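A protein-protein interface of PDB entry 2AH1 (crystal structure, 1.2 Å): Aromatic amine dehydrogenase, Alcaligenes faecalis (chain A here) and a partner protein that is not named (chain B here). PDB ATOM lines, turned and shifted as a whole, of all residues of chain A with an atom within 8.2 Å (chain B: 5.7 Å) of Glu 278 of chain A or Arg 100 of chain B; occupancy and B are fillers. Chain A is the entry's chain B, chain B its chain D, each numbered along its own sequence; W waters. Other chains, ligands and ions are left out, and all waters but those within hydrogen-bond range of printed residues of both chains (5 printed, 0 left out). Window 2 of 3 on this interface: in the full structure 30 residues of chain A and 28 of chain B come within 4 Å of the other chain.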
ATOM      1  N   TYR A 109      19.893 -13.673  10.818  1.00  0.00           N
ATOM      2  CA  TYR A 109      18.463 -13.433  10.912  1.00  0.00           C
ATOM      3  C   TYR A 109      17.715 -14.751  10.761  1.00  0.00           C
ATOM      4  O   TYR A 109      18.071 -15.573   9.921  1.00  0.00           O
ATOM      5  CB  TYR A 109      18.025 -12.485   9.800  1.00  0.00           C
ATOM      6  CG  TYR A 109      18.542 -11.065   9.872  1.00  0.00           C
ATOM      7  CD1 TYR A 109      19.671 -10.669   9.165  1.00  0.00           C
ATOM      8  CD2 TYR A 109      17.892 -10.112  10.636  1.00  0.00           C
ATOM      9  CE1 TYR A 109      20.136  -9.356   9.225  1.00  0.00           C
ATOM     10  CE2 TYR A 109      18.348  -8.822  10.705  1.00  0.00           C
ATOM     11  CZ  TYR A 109      19.459  -8.426  10.000  1.00  0.00           C
ATOM     12  OH  TYR A 109      19.891  -7.121  10.075  1.00  0.00           O
ATOM     13  N   TRP A 154      13.538 -10.852  -0.182  1.00  0.00           N
ATOM     14  CA  TRP A 154      14.479 -11.261   0.860  1.00  0.00           C
ATOM     15  C   TRP A 154      13.763 -11.825   2.061  1.00  0.00           C
ATOM     16  O   TRP A 154      12.822 -11.230   2.607  1.00  0.00           O
ATOM     17  CB  TRP A 154      15.306 -10.057   1.280  1.00  0.00           C
ATOM     18  CG  TRP A 154      16.543 -10.410   2.020  1.00  0.00           C
ATOM     19  CD1 TRP A 154      16.826 -10.130   3.323  1.00  0.00           C
ATOM     20  CD2 TRP A 154      17.675 -11.100   1.504  1.00  0.00           C
ATOM     21  NE1 TRP A 154      18.071 -10.613   3.649  1.00  0.00           N
ATOM     22  CE2 TRP A 154      18.614 -11.213   2.548  1.00  0.00           C
ATOM     23  CE3 TRP A 154      17.992 -11.644   0.264  1.00  0.00           C
ATOM     24  CZ2 TRP A 154      19.848 -11.847   2.379  1.00  0.00           C
ATOM     25  CZ3 TRP A 154      19.203 -12.259   0.098  1.00  0.00           C
ATOM     26  CH2 TRP A 154      20.117 -12.365   1.153  1.00  0.00           C
ATOM     27  N   SER A 197       6.247   1.882   2.329  1.00  0.00           N
ATOM     28  CA  SER A 197       7.096   2.629   1.403  1.00  0.00           C
ATOM     29  C   SER A 197       8.540   2.257   1.673  1.00  0.00           C
ATOM     30  O   SER A 197       9.070   2.494   2.760  1.00  0.00           O
ATOM     31  CB  SER A 197       6.947   4.127   1.589  1.00  0.00           C
ATOM     32  OG  SER A 197       7.893   4.811   0.797  1.00  0.00           O
ATOM     33  N   VAL A 198       9.170   1.672   0.677  1.00  0.00           N
ATOM     34  CA  VAL A 198      10.571   1.297   0.810  1.00  0.00           C
ATOM     35  C   VAL A 198      11.430   2.533   1.062  1.00  0.00           C
ATOM     36  O   VAL A 198      12.312   2.512   1.913  1.00  0.00           O
ATOM     37  CB  VAL A 198      11.025   0.497  -0.412  1.00  0.00           C
ATOM     38  CG1 VAL A 198      12.528   0.360  -0.459  1.00  0.00           C
ATOM     39  CG2 VAL A 198      10.359  -0.870  -0.396  1.00  0.00           C
ATOM     40  N   LYS A 199      11.160   3.618   0.323  1.00  0.00           N
ATOM     41  CA  LYS A 199      11.924   4.859   0.446  1.00  0.00           C
ATOM     42  C   LYS A 199      11.650   5.581   1.763  1.00  0.00           C
ATOM     43  O   LYS A 199      12.584   6.044   2.421  1.00  0.00           O
ATOM     44  CB  LYS A 199      11.608   5.807  -0.747  1.00  0.00           C
ATOM     45  N   ASP A 200      10.379   5.683   2.142  1.00  0.00           N
ATOM     46  CA  ASP A 200       9.965   6.572   3.246  1.00  0.00           C
ATOM     47  C   ASP A 200       9.807   5.908   4.592  1.00  0.00           C
ATOM     48  O   ASP A 200       9.884   6.588   5.623  1.00  0.00           O
ATOM     49  CB  ASP A 200       8.643   7.266   2.933  1.00  0.00           C
ATOM     50  CG  ASP A 200       8.725   8.169   1.749  1.00  0.00           C
ATOM     51  OD1 ASP A 200       9.831   8.637   1.394  1.00  0.00           O
ATOM     52  OD2 ASP A 200       7.703   8.472   1.107  1.00  0.00           O
ATOM     53  N   ASP A 201       9.584   4.600   4.610  1.00  0.00           N
ATOM     54  CA  ASP A 201       9.382   3.917   5.890  1.00  0.00           C
ATOM     55  C   ASP A 201       9.816   2.448   5.875  1.00  0.00           C
ATOM     56  O   ASP A 201       9.009   1.544   6.099  1.00  0.00           O
ATOM     57  CB  ASP A 201       7.922   4.063   6.328  1.00  0.00           C
ATOM     58  CG  ASP A 201       7.722   3.868   7.831  1.00  0.00           C
ATOM     59  OD1 ASP A 201       8.708   3.967   8.612  1.00  0.00           O
ATOM     60  OD2 ASP A 201       6.605   3.614   8.317  1.00  0.00           O
ATOM     61  N   PRO A 202      11.096   2.210   5.611  1.00  0.00           N
ATOM     62  CA  PRO A 202      11.544   0.838   5.438  1.00  0.00           C
ATOM     63  C   PRO A 202      11.320   0.052   6.712  1.00  0.00           C
ATOM     64  O   PRO A 202      11.553   0.586   7.796  1.00  0.00           O
ATOM     65  CB  PRO A 202      13.037   0.991   5.155  1.00  0.00           C
ATOM     66  CG  PRO A 202      13.406   2.326   5.689  1.00  0.00           C
ATOM     67  CD  PRO A 202      12.203   3.171   5.461  1.00  0.00           C
ATOM     68  N   ILE A 203      10.862  -1.189   6.575  1.00  0.00           N
ATOM     69  CA  ILE A 203      10.688  -2.100   7.707  1.00  0.00           C
ATOM     70  C   ILE A 203      11.911  -2.986   7.976  1.00  0.00           C
ATOM     71  O   ILE A 203      12.710  -3.290   7.079  1.00  0.00           O
ATOM     72  CB  ILE A 203       9.478  -3.045   7.523  1.00  0.00           C
ATOM     73  CG1 ILE A 203       9.601  -3.868   6.246  1.00  0.00           C
ATOM     74  CG2 ILE A 203       8.144  -2.282   7.631  1.00  0.00           C
ATOM     75  CD1 ILE A 203       8.755  -5.068   6.300  1.00  0.00           C
ATOM     76  N   ILE A 205      13.214  -6.706   8.692  1.00  0.00           N
ATOM     77  CA  ILE A 205      12.691  -7.935   8.116  1.00  0.00           C
ATOM     78  C   ILE A 205      12.146  -8.909   9.165  1.00  0.00           C
ATOM     79  O   ILE A 205      11.350  -9.776   8.848  1.00  0.00           O
ATOM     80  CB  ILE A 205      13.751  -8.643   7.220  1.00  0.00           C
ATOM     81  CG1 ILE A 205      14.950  -9.150   8.043  1.00  0.00           C
ATOM     82  CG2 ILE A 205      14.148  -7.742   6.040  1.00  0.00           C
ATOM     83  CD1 ILE A 205      15.835 -10.160   7.296  1.00  0.00           C
ATOM     84  N   TYR A 219      11.925   1.506  10.527  1.00  0.00           N
ATOM     85  CA  TYR A 219      13.047   2.319  10.971  1.00  0.00           C
ATOM     86  C   TYR A 219      12.614   3.525  11.810  1.00  0.00           C
ATOM     87  O   TYR A 219      13.363   3.968  12.681  1.00  0.00           O
ATOM     88  CB  TYR A 219      13.836   2.836   9.779  1.00  0.00           C
ATOM     89  CG  TYR A 219      14.859   1.903   9.168  1.00  0.00           C
ATOM     90  CD1 TYR A 219      16.058   2.407   8.711  1.00  0.00           C
ATOM     91  CD2 TYR A 219      14.623   0.533   9.035  1.00  0.00           C
ATOM     92  CE1 TYR A 219      17.010   1.584   8.139  1.00  0.00           C
ATOM     93  CE2 TYR A 219      15.579  -0.304   8.459  1.00  0.00           C
ATOM     94  CZ  TYR A 219      16.766   0.233   8.018  1.00  0.00           C
ATOM     95  OH  TYR A 219      17.713  -0.589   7.439  1.00  0.00           O
ATOM     96  N   TYR A 220      11.416   4.053  11.537  1.00  0.00           N
ATOM     97  CA  TYR A 220      10.902   5.243  12.228  1.00  0.00           C
ATOM     98  C   TYR A 220       9.873   4.898  13.300  1.00  0.00           C
ATOM     99  O   TYR A 220       9.201   5.784  13.846  1.00  0.00           O
ATOM    100  CB  TYR A 220      10.354   6.225  11.186  1.00  0.00           C
ATOM    101  CG  TYR A 220      11.388   6.568  10.147  1.00  0.00           C
ATOM    102  CD1 TYR A 220      11.235   6.176   8.819  1.00  0.00           C
ATOM    103  CD2 TYR A 220      12.530   7.278  10.484  1.00  0.00           C
ATOM    104  CE1 TYR A 220      12.185   6.484   7.867  1.00  0.00           C
ATOM    105  CE2 TYR A 220      13.491   7.594   9.531  1.00  0.00           C
ATOM    106  CZ  TYR A 220      13.312   7.190   8.221  1.00  0.00           C
ATOM    107  OH  TYR A 220      14.248   7.492   7.263  1.00  0.00           O
ATOM    108  N   VAL A 252      13.230   5.056  18.499  1.00  0.00           N
ATOM    109  CA  VAL A 252      13.023   4.207  17.308  1.00  0.00           C
ATOM    110  C   VAL A 252      13.467   2.780  17.641  1.00  0.00           C
ATOM    111  O   VAL A 252      14.181   2.570  18.616  1.00  0.00           O
ATOM    112  CB  VAL A 252      13.804   4.739  16.074  1.00  0.00           C
ATOM    113  CG1 VAL A 252      13.336   6.154  15.714  1.00  0.00           C
ATOM    114  CG2 VAL A 252      15.302   4.734  16.319  1.00  0.00           C
ATOM    115  N   ASP A 275      16.980   8.988  20.693  1.00  0.00           N
ATOM    116  CA  ASP A 275      17.852   9.777  19.830  1.00  0.00           C
ATOM    117  C   ASP A 275      18.099   9.100  18.487  1.00  0.00           C
ATOM    118  O   ASP A 275      19.206   9.139  17.951  1.00  0.00           O
ATOM    119  CB  ASP A 275      19.168  10.104  20.531  1.00  0.00           C
ATOM    120  CG  ASP A 275      18.953  10.694  21.913  1.00  0.00           C
ATOM    121  OD1 ASP A 275      18.018  11.506  22.053  1.00  0.00           O
ATOM    122  OD2 ASP A 275      19.658  10.407  22.910  1.00  0.00           O
ATOM    123  N   GLY A 276      17.044   8.502  17.957  1.00  0.00           N
ATOM    124  CA  GLY A 276      17.077   7.924  16.621  1.00  0.00           C
ATOM    125  C   GLY A 276      17.371   8.923  15.535  1.00  0.00           C
ATOM    126  O   GLY A 276      16.934  10.066  15.592  1.00  0.00           O
ATOM    127  N   LYS A 277      18.115   8.476  14.542  1.00  0.00           N
ATOM    128  CA  LYS A 277      18.394   9.244  13.353  1.00  0.00           C
ATOM    129  C   LYS A 277      18.920   8.232  12.335  1.00  0.00           C
ATOM    130  O   LYS A 277      19.079   7.038  12.662  1.00  0.00           O
ATOM    131  CB  LYS A 277      19.423  10.337  13.633  1.00  0.00           C
ATOM    132  CG  LYS A 277      20.765   9.861  14.137  1.00  0.00           C
ATOM    133  CD  LYS A 277      21.709  11.020  14.409  1.00  0.00           C
ATOM    134  CE  LYS A 277      23.167  10.612  14.211  1.00  0.00           C
ATOM    135  NZ  LYS A 277      24.129  11.758  14.123  1.00  0.00           N
ATOM    136  N   GLU A 278      19.192   8.710  11.130  1.00  0.00           N
ATOM    137  CA  GLU A 278      19.735   7.874  10.090  1.00  0.00           C
ATOM    138  C   GLU A 278      20.989   7.168  10.604  1.00  0.00           C
ATOM    139  O   GLU A 278      21.903   7.818  11.070  1.00  0.00           O
ATOM    140  CB  GLU A 278      20.071   8.706   8.858  1.00  0.00           C
ATOM    141  CG  GLU A 278      20.608   7.889   7.695  1.00  0.00           C
ATOM    142  CD  GLU A 278      19.640   6.826   7.243  1.00  0.00           C
ATOM    143  OE1 GLU A 278      18.538   7.197   6.769  1.00  0.00           O
ATOM    144  OE2 GLU A 278      19.987   5.611   7.354  1.00  0.00           O
ATOM    145  N   GLY A 279      21.016   5.838  10.503  1.00  0.00           N
ATOM    146  CA  GLY A 279      22.176   5.040  10.928  1.00  0.00           C
ATOM    147  C   GLY A 279      22.092   4.356  12.280  1.00  0.00           C
ATOM    148  O   GLY A 279      23.048   3.697  12.684  1.00  0.00           O
ATOM    149  N   THR A 280      20.972   4.474  12.985  1.00  0.00           N
ATOM    150  CA  THR A 280      20.872   3.904  14.328  1.00  0.00           C
ATOM    151  C   THR A 280      20.018   2.640  14.378  1.00  0.00           C
ATOM    152  O   THR A 280      19.674   2.143  15.445  1.00  0.00           O
ATOM    153  CB  THR A 280      20.416   4.968  15.395  1.00  0.00           C
ATOM    154  OG1 THR A 280      18.997   5.169  15.350  1.00  0.00           O
ATOM    155  CG2 THR A 280      21.115   6.315  15.184  1.00  0.00           C
ATOM    156  N   HIS A 281      19.680   2.081  13.223  1.00  0.00           N
ATOM    157  CA  HIS A 281      18.725   0.986  13.191  1.00  0.00           C
ATOM    158  C   HIS A 281      19.248  -0.341  13.736  1.00  0.00           C
ATOM    159  O   HIS A 281      18.466  -1.246  13.973  1.00  0.00           O
ATOM    160  CB  HIS A 281      18.121   0.787  11.797  1.00  0.00           C
ATOM    161  CG  HIS A 281      19.113   0.724  10.676  1.00  0.00           C
ATOM    162  ND1 HIS A 281      19.748   1.836  10.172  1.00  0.00           N
ATOM    163  CD2 HIS A 281      19.561  -0.332   9.948  1.00  0.00           C
ATOM    164  CE1 HIS A 281      20.544   1.468   9.184  1.00  0.00           C
ATOM    165  NE2 HIS A 281      20.449   0.158   9.028  1.00  0.00           N
ATOM    166  N   LYS A 282      20.559  -0.444  13.924  1.00  0.00           N
ATOM    167  CA  LYS A 282      21.142  -1.651  14.509  1.00  0.00           C
ATOM    168  C   LYS A 282      21.726  -1.411  15.913  1.00  0.00           C
ATOM    169  O   LYS A 282      22.472  -2.232  16.452  1.00  0.00           O
ATOM    170  CB  LYS A 282      22.160  -2.264  13.528  1.00  0.00           C
ATOM    171  CG  LYS A 282      21.473  -2.849  12.293  1.00  0.00           C
ATOM    172  CD  LYS A 282      22.440  -3.151  11.211  1.00  0.00           C
ATOM    173  CE  LYS A 282      21.739  -3.457   9.892  1.00  0.00           C
ATOM    174  NZ  LYS A 282      22.727  -3.650   8.811  1.00  0.00           N
ATOM    175  N   PHE A 283      21.355  -0.282  16.516  1.00  0.00           N
ATOM    176  CA  PHE A 283      21.840   0.056  17.855  1.00  0.00           C
ATOM    177  C   PHE A 283      21.266  -0.904  18.898  1.00  0.00           C
ATOM    178  O   PHE A 283      20.119  -1.340  18.815  1.00  0.00           O
ATOM    179  CB  PHE A 283      21.449   1.489  18.266  1.00  0.00           C
ATOM    180  CG  PHE A 283      22.395   2.558  17.808  1.00  0.00           C
ATOM    181  CD1 PHE A 283      23.219   2.392  16.708  1.00  0.00           C
ATOM    182  CD2 PHE A 283      22.446   3.784  18.491  1.00  0.00           C
ATOM    183  CE1 PHE A 283      24.086   3.417  16.297  1.00  0.00           C
ATOM    184  CE2 PHE A 283      23.303   4.777  18.083  1.00  0.00           C
ATOM    185  CZ  PHE A 283      24.119   4.603  16.993  1.00  0.00           C
ATOM    186  N   GLN B  96      26.203   2.374   9.724  1.00  0.00           N
ATOM    187  CA  GLN B  96      24.973   1.998   9.053  1.00  0.00           C
ATOM    188  C   GLN B  96      24.254   3.175   8.381  1.00  0.00           C
ATOM    189  O   GLN B  96      23.060   3.111   8.132  1.00  0.00           O
ATOM    190  CB  GLN B  96      24.060   1.306  10.074  1.00  0.00           C
ATOM    191  CG  GLN B  96      24.666   0.016  10.717  1.00  0.00           C
ATOM    192  CD  GLN B  96      24.757  -1.113   9.717  1.00  0.00           C
ATOM    193  OE1 GLN B  96      25.608  -2.028   9.831  1.00  0.00           O
ATOM    194  NE2 GLN B  96      23.900  -1.075   8.744  1.00  0.00           N
ATOM    195  N   THR B  97      24.982   4.237   8.091  1.00  0.00           N
ATOM    196  CA  THR B  97      24.363   5.397   7.445  1.00  0.00           C
ATOM    197  C   THR B  97      23.766   4.994   6.110  1.00  0.00           C
ATOM    198  O   THR B  97      24.485   4.539   5.240  1.00  0.00           O
ATOM    199  CB  THR B  97      25.400   6.473   7.260  1.00  0.00           C
ATOM    200  OG1 THR B  97      25.790   6.940   8.554  1.00  0.00           O
ATOM    201  CG2 THR B  97      24.797   7.704   6.549  1.00  0.00           C
ATOM    202  N   ARG B  98      22.446   5.168   5.981  1.00  0.00           N
ATOM    203  CA  ARG B  98      21.682   4.949   4.739  1.00  0.00           C
ATOM    204  C   ARG B  98      21.585   3.463   4.358  1.00  0.00           C
ATOM    205  O   ARG B  98      21.131   3.143   3.269  1.00  0.00           O
ATOM    206  CB  ARG B  98      22.205   5.825   3.581  1.00  0.00           C
ATOM    207  CG  ARG B  98      21.880   7.306   3.749  1.00  0.00           C
ATOM    208  CD  ARG B  98      20.477   7.644   3.364  1.00  0.00           C
ATOM    209  NE  ARG B  98      20.233   7.510   1.923  1.00  0.00           N
ATOM    210  CZ  ARG B  98      20.461   8.446   1.007  1.00  0.00           C
ATOM    211  NH1 ARG B  98      20.957   9.631   1.348  1.00  0.00           N
ATOM    212  NH2 ARG B  98      20.191   8.188  -0.268  1.00  0.00           N
ATOM    213  N   GLU B  99      22.007   2.566   5.267  1.00  0.00           N
ATOM    214  CA  GLU B  99      21.981   1.133   5.020  1.00  0.00           C
ATOM    215  C   GLU B  99      20.563   0.624   5.118  1.00  0.00           C
ATOM    216  O   GLU B  99      19.787   1.035   5.991  1.00  0.00           O
ATOM    217  CB  GLU B  99      22.891   0.425   6.020  1.00  0.00           C
ATOM    218  CG  GLU B  99      23.153  -1.048   5.703  1.00  0.00           C
ATOM    219  CD  GLU B  99      22.111  -2.019   6.238  1.00  0.00           C
ATOM    220  OE1 GLU B  99      21.154  -1.601   6.927  1.00  0.00           O
ATOM    221  OE2 GLU B  99      22.252  -3.247   5.984  1.00  0.00           O
ATOM    222  N   ARG B 100      20.199  -0.275   4.209  1.00  0.00           N
ATOM    223  CA  ARG B 100      18.858  -0.811   4.164  1.00  0.00           C
ATOM    224  C   ARG B 100      18.879  -2.332   4.128  1.00  0.00           C
ATOM    225  O   ARG B 100      19.917  -2.912   3.826  1.00  0.00           O
ATOM    226  CB  ARG B 100      18.107  -0.199   2.977  1.00  0.00           C
ATOM    227  CG  ARG B 100      17.882   1.330   3.124  1.00  0.00           C
ATOM    228  CD  ARG B 100      16.968   1.704   4.285  1.00  0.00           C
ATOM    229  NE  ARG B 100      16.724   3.142   4.382  1.00  0.00           N
ATOM    230  CZ  ARG B 100      17.452   4.011   5.089  1.00  0.00           C
ATOM    231  NH1 ARG B 100      18.501   3.624   5.798  1.00  0.00           N
ATOM    232  NH2 ARG B 100      17.116   5.294   5.097  1.00  0.00           N
ATOM    233  N   PRO B 101      17.756  -2.963   4.450  1.00  0.00           N
ATOM    234  CA  PRO B 101      17.708  -4.437   4.500  1.00  0.00           C
ATOM    235  C   PRO B 101      17.809  -5.125   3.149  1.00  0.00           C
ATOM    236  O   PRO B 101      17.862  -4.470   2.102  1.00  0.00           O
ATOM    237  CB  PRO B 101      16.367  -4.725   5.154  1.00  0.00           C
ATOM    238  CG  PRO B 101      16.022  -3.408   5.821  1.00  0.00           C
ATOM    239  CD  PRO B 101      16.463  -2.364   4.837  1.00  0.00           C
ATOM    240  N   GLY B 102      17.825  -6.461   3.169  1.00  0.00           N
ATOM    241  CA  GLY B 102      18.151  -7.246   1.991  1.00  0.00           C
ATOM    242  C   GLY B 102      17.181  -7.122   0.826  1.00  0.00           C
ATOM    243  O   GLY B 102      17.508  -7.535  -0.281  1.00  0.00           O
ATOM    244  N   GLU B 104      16.502  -4.302  -0.370  1.00  0.00           N
ATOM    245  CA  GLU B 104      17.228  -3.304  -1.157  1.00  0.00           C
ATOM    246  C   GLU B 104      18.681  -3.793  -1.180  1.00  0.00           C
ATOM    247  O   GLU B 104      19.562  -3.249  -0.517  1.00  0.00           O
ATOM    248  CB  GLU B 104      17.112  -1.928  -0.507  1.00  0.00           C
ATOM    249  CG  GLU B 104      15.685  -1.420  -0.315  1.00  0.00           C
ATOM    250  CD  GLU B 104      15.654  -0.035   0.311  1.00  0.00           C
ATOM    251  OE1 GLU B 104      16.149   0.892  -0.330  1.00  0.00           O
ATOM    252  OE2 GLU B 104      15.138   0.113   1.448  1.00  0.00           O
ATOM    253  N   LEU B 107      22.161  -2.076  -1.058  1.00  0.00           N
ATOM    254  CA  LEU B 107      22.343  -1.094   0.004  1.00  0.00           C
ATOM    255  C   LEU B 107      22.540  -1.783   1.351  1.00  0.00           C
ATOM    256  O   LEU B 107      22.555  -1.132   2.388  1.00  0.00           O
ATOM    257  CB  LEU B 107      21.105  -0.179   0.084  1.00  0.00           C
ATOM    258  CG  LEU B 107      20.754   0.629  -1.161  1.00  0.00           C
ATOM    259  CD1 LEU B 107      19.569   1.560  -0.910  1.00  0.00           C
ATOM    260  CD2 LEU B 107      21.932   1.386  -1.656  1.00  0.00           C
ATOM    261  N   HIS B 108      22.682  -3.109   1.335  1.00  0.00           N
ATOM    262  CA  HIS B 108      22.621  -3.908   2.549  1.00  0.00           C
ATOM    263  C   HIS B 108      23.996  -4.425   2.949  1.00  0.00           C
ATOM    264  O   HIS B 108      24.737  -4.927   2.107  1.00  0.00           O
ATOM    265  CB  HIS B 108      21.672  -5.091   2.297  1.00  0.00           C
ATOM    266  CG  HIS B 108      21.426  -5.923   3.512  1.00  0.00           C
ATOM    267  ND1 HIS B 108      21.446  -7.301   3.538  1.00  0.00           N
ATOM    268  CD2 HIS B 108      21.138  -5.525   4.764  1.00  0.00           C
ATOM    269  CE1 HIS B 108      21.190  -7.718   4.769  1.00  0.00           C
ATOM    270  NE2 HIS B 108      21.002  -6.651   5.528  1.00  0.00           N
ATOM    271  N   ASN B 109      24.337  -4.324   4.236  1.00  0.00           N
ATOM    272  CA  ASN B 109      25.692  -4.714   4.675  1.00  0.00           C
ATOM    273  C   ASN B 109      25.767  -5.854   5.702  1.00  0.00           C
ATOM    274  O   ASN B 109      26.810  -6.068   6.283  1.00  0.00           O
ATOM    275  CB  ASN B 109      26.540  -3.509   5.127  1.00  0.00           C
ATOM    276  CG  ASN B 109      26.137  -2.934   6.451  1.00  0.00           C
ATOM    277  OD1 ASN B 109      25.335  -3.509   7.179  1.00  0.00           O
ATOM    278  ND2 ASN B 109      26.706  -1.761   6.781  1.00  0.00           N
HETATM  279  O   HOH W   1      14.173   5.798   4.754  1.00  0.00           O
HETATM  280  O   HOH W   2      25.758   3.879  12.227  1.00  0.00           O
HETATM  281  O   HOH W   3      19.228  -3.407   7.402  1.00  0.00           O
HETATM  282  O   HOH W   4      18.464  -6.039   7.820  1.00  0.00           O
HETATM  283  O   HOH W   5      14.875   2.707   2.030  1.00  0.00           O
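Among the printed residues, pairs that only touch across the chains: Trp 154 of chain A with Gly 102 of chain B (3.4 Å), Val 198 of chain A with Glu 104 of chain B (3.2 Å), Pro 202 of chain A with Arg 100 of chain B (3.7 Å), Ile 203 of chain A with Pro 101 of chain B (3.5 Å), Ile 205 of chain A with Pro 101 of chain B (3.8 Å), Tyr 219 of chain A with Arg 100 of chain B (3.4 Å), Tyr 219 of chain A with Pro 101 of chain B (3.4 Å), Gly 279 of chain A with Gln 96 of chain B (3.5 Å) and His 281 of chain A with Gln 96 of chain B (3.2 Å).
OE1 of Glu 99 of chain B lies close to NE2 of Gln 96 of chain B (3.3 Å). The side-chain amide oxygen (OE1) of Gln 96 of chain B sits close to the side-chain amide oxygen (OD1) of Asn 109 of chain B. The backbone NH of Asn 109 of chain B sits at hydrogen-bond distance from the side-chain carboxylate of Glu 99 of chain B (2.9 Å). N of Arg 100 of chain B is in hydrogen-bond range of O of Leu 107 of chain B, 3.1 Å away. The backbone carbonyl oxygen of Pro 202 of chain A lies within hydrogen-bond range of the backbone NH of Tyr 219 of chain A (2.9 Å). The side-chain hydroxyl (OH) of Tyr 219 of chain A lies close to a ring nitrogen (NE2) of His 281 of chain A (3.3 Å).
NE2 of Gln 96 of chain B lies close to NZ of Lys 282 of chain A (2.8 Å). N of Arg 98 of chain B lies within hydrogen-bond range of OE2 of Glu 278 of chain A, at 2.9 Å. O of Glu 99 of chain B sits at hydrogen-bond distance from OH of Tyr 219 of chain A (3.0 Å). The side-chain carboxylate (OE1) of Glu 99 of chain B is in hydrogen-bond range of a ring nitrogen (NE2) of His 281 of chain A, 2.8 Å away. The side-chain carboxylate (OE2) of Glu 99 of chain B lies within salt-bridge range of the side-chain amino group (NZ) of Lys 282 of chain A (2.9 Å). The guanidinium group (NH2) of Arg 100 of chain B lies within salt-bridge range of the side-chain carboxylate (OE1) of Glu 278 of chain A. OD1 of Asn 109 of chain B is in hydrogen-bond range of NZ of Lys 282 of chain A (3.1 Å).
Of the 11 printed residues of chain B, 8 touch a printed residue of chain A. Printed residues of chain B that touch a printed residue of chain A: Gln 96, Arg 98, Glu 99, Arg 100, Pro 101, Gly 102, Glu 104 and Asn 109. Hydrophobic or aromatic side chains of chain B within 4 Å of the printed part of chain A: Pro 101. Hydrophobic or aromatic side chains of chain A that line the printed part of chain B: Trp 154, Val 198, Pro 202, Ile 205, Tyr 219 and His 281. Along chain A the printed residues that touch a printed residue of chain B span positions 154 to 282. Among the printed residues, 16 pairs touch across the chains. Among the printed residues, Asp or Glu carboxylates within 4 Å of a Lys or Arg side-chain nitrogen of the other chain: Glu 278 of chain A with Arg 100 of chain B (2.9 Å) and Lys 282 of chain A with Glu 99 of chain B (2.9 Å).
Of the printed residues of chain B, Tyr 219 of chain A touches Glu 99, Arg 100 and Pro 101. Lys 277 of chain A touches none of the printed residues of chain B. Glu 278 of chain A touches two residues of chain B. Phe 283 of chain A touches none of the printed residues of chain B. Glu 99 of chain B touches just these residues of chain A: Tyr 219, His 281 and Lys 282. Of the printed residues of chain A, Pro 101 of chain B touches Ile 203, Ile 205 and Tyr 219. Printed residues of chain A within 4 Å of Glu 104 of chain B: Val 198 (3.2 Å). The nearest printed residue of chain B that does not touch Glu 278 of chain A is Thr 97 of chain B (4.03 Å). The nearest residue of chain A that does not touch Arg 100 of chain B is Tyr 220 of chain A (4.2 Å).
Water W5 lies within hydrogen-bond range of O of Val 198 of chain A, OE2 of Glu 104 of chain B and NE of Arg 100 of chain B. Water W3 bridges OE1 of Glu 99 of chain B (2.7 Å) and OH of Tyr 219 of chain A (3.2 Å). Water W2 lies within hydrogen-bond range of O of Gly 279 of chain A (2.8 Å) and N of Gln 96 of chain B (3.0 Å). Water W1 lies within hydrogen-bond range of the backbone carbonyl oxygen of Lys 199 of chain A (2.8 Å), the guanidinium group of Arg 100 of chain B (3.0 Å) and the side-chain hydroxyl of Tyr 220 of chain A (3.0 Å). Water W4 lies within hydrogen-bond range of OH of Tyr 109 of chain A (2.9 Å) and NE2 of His 108 of chain B (3.5 Å).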
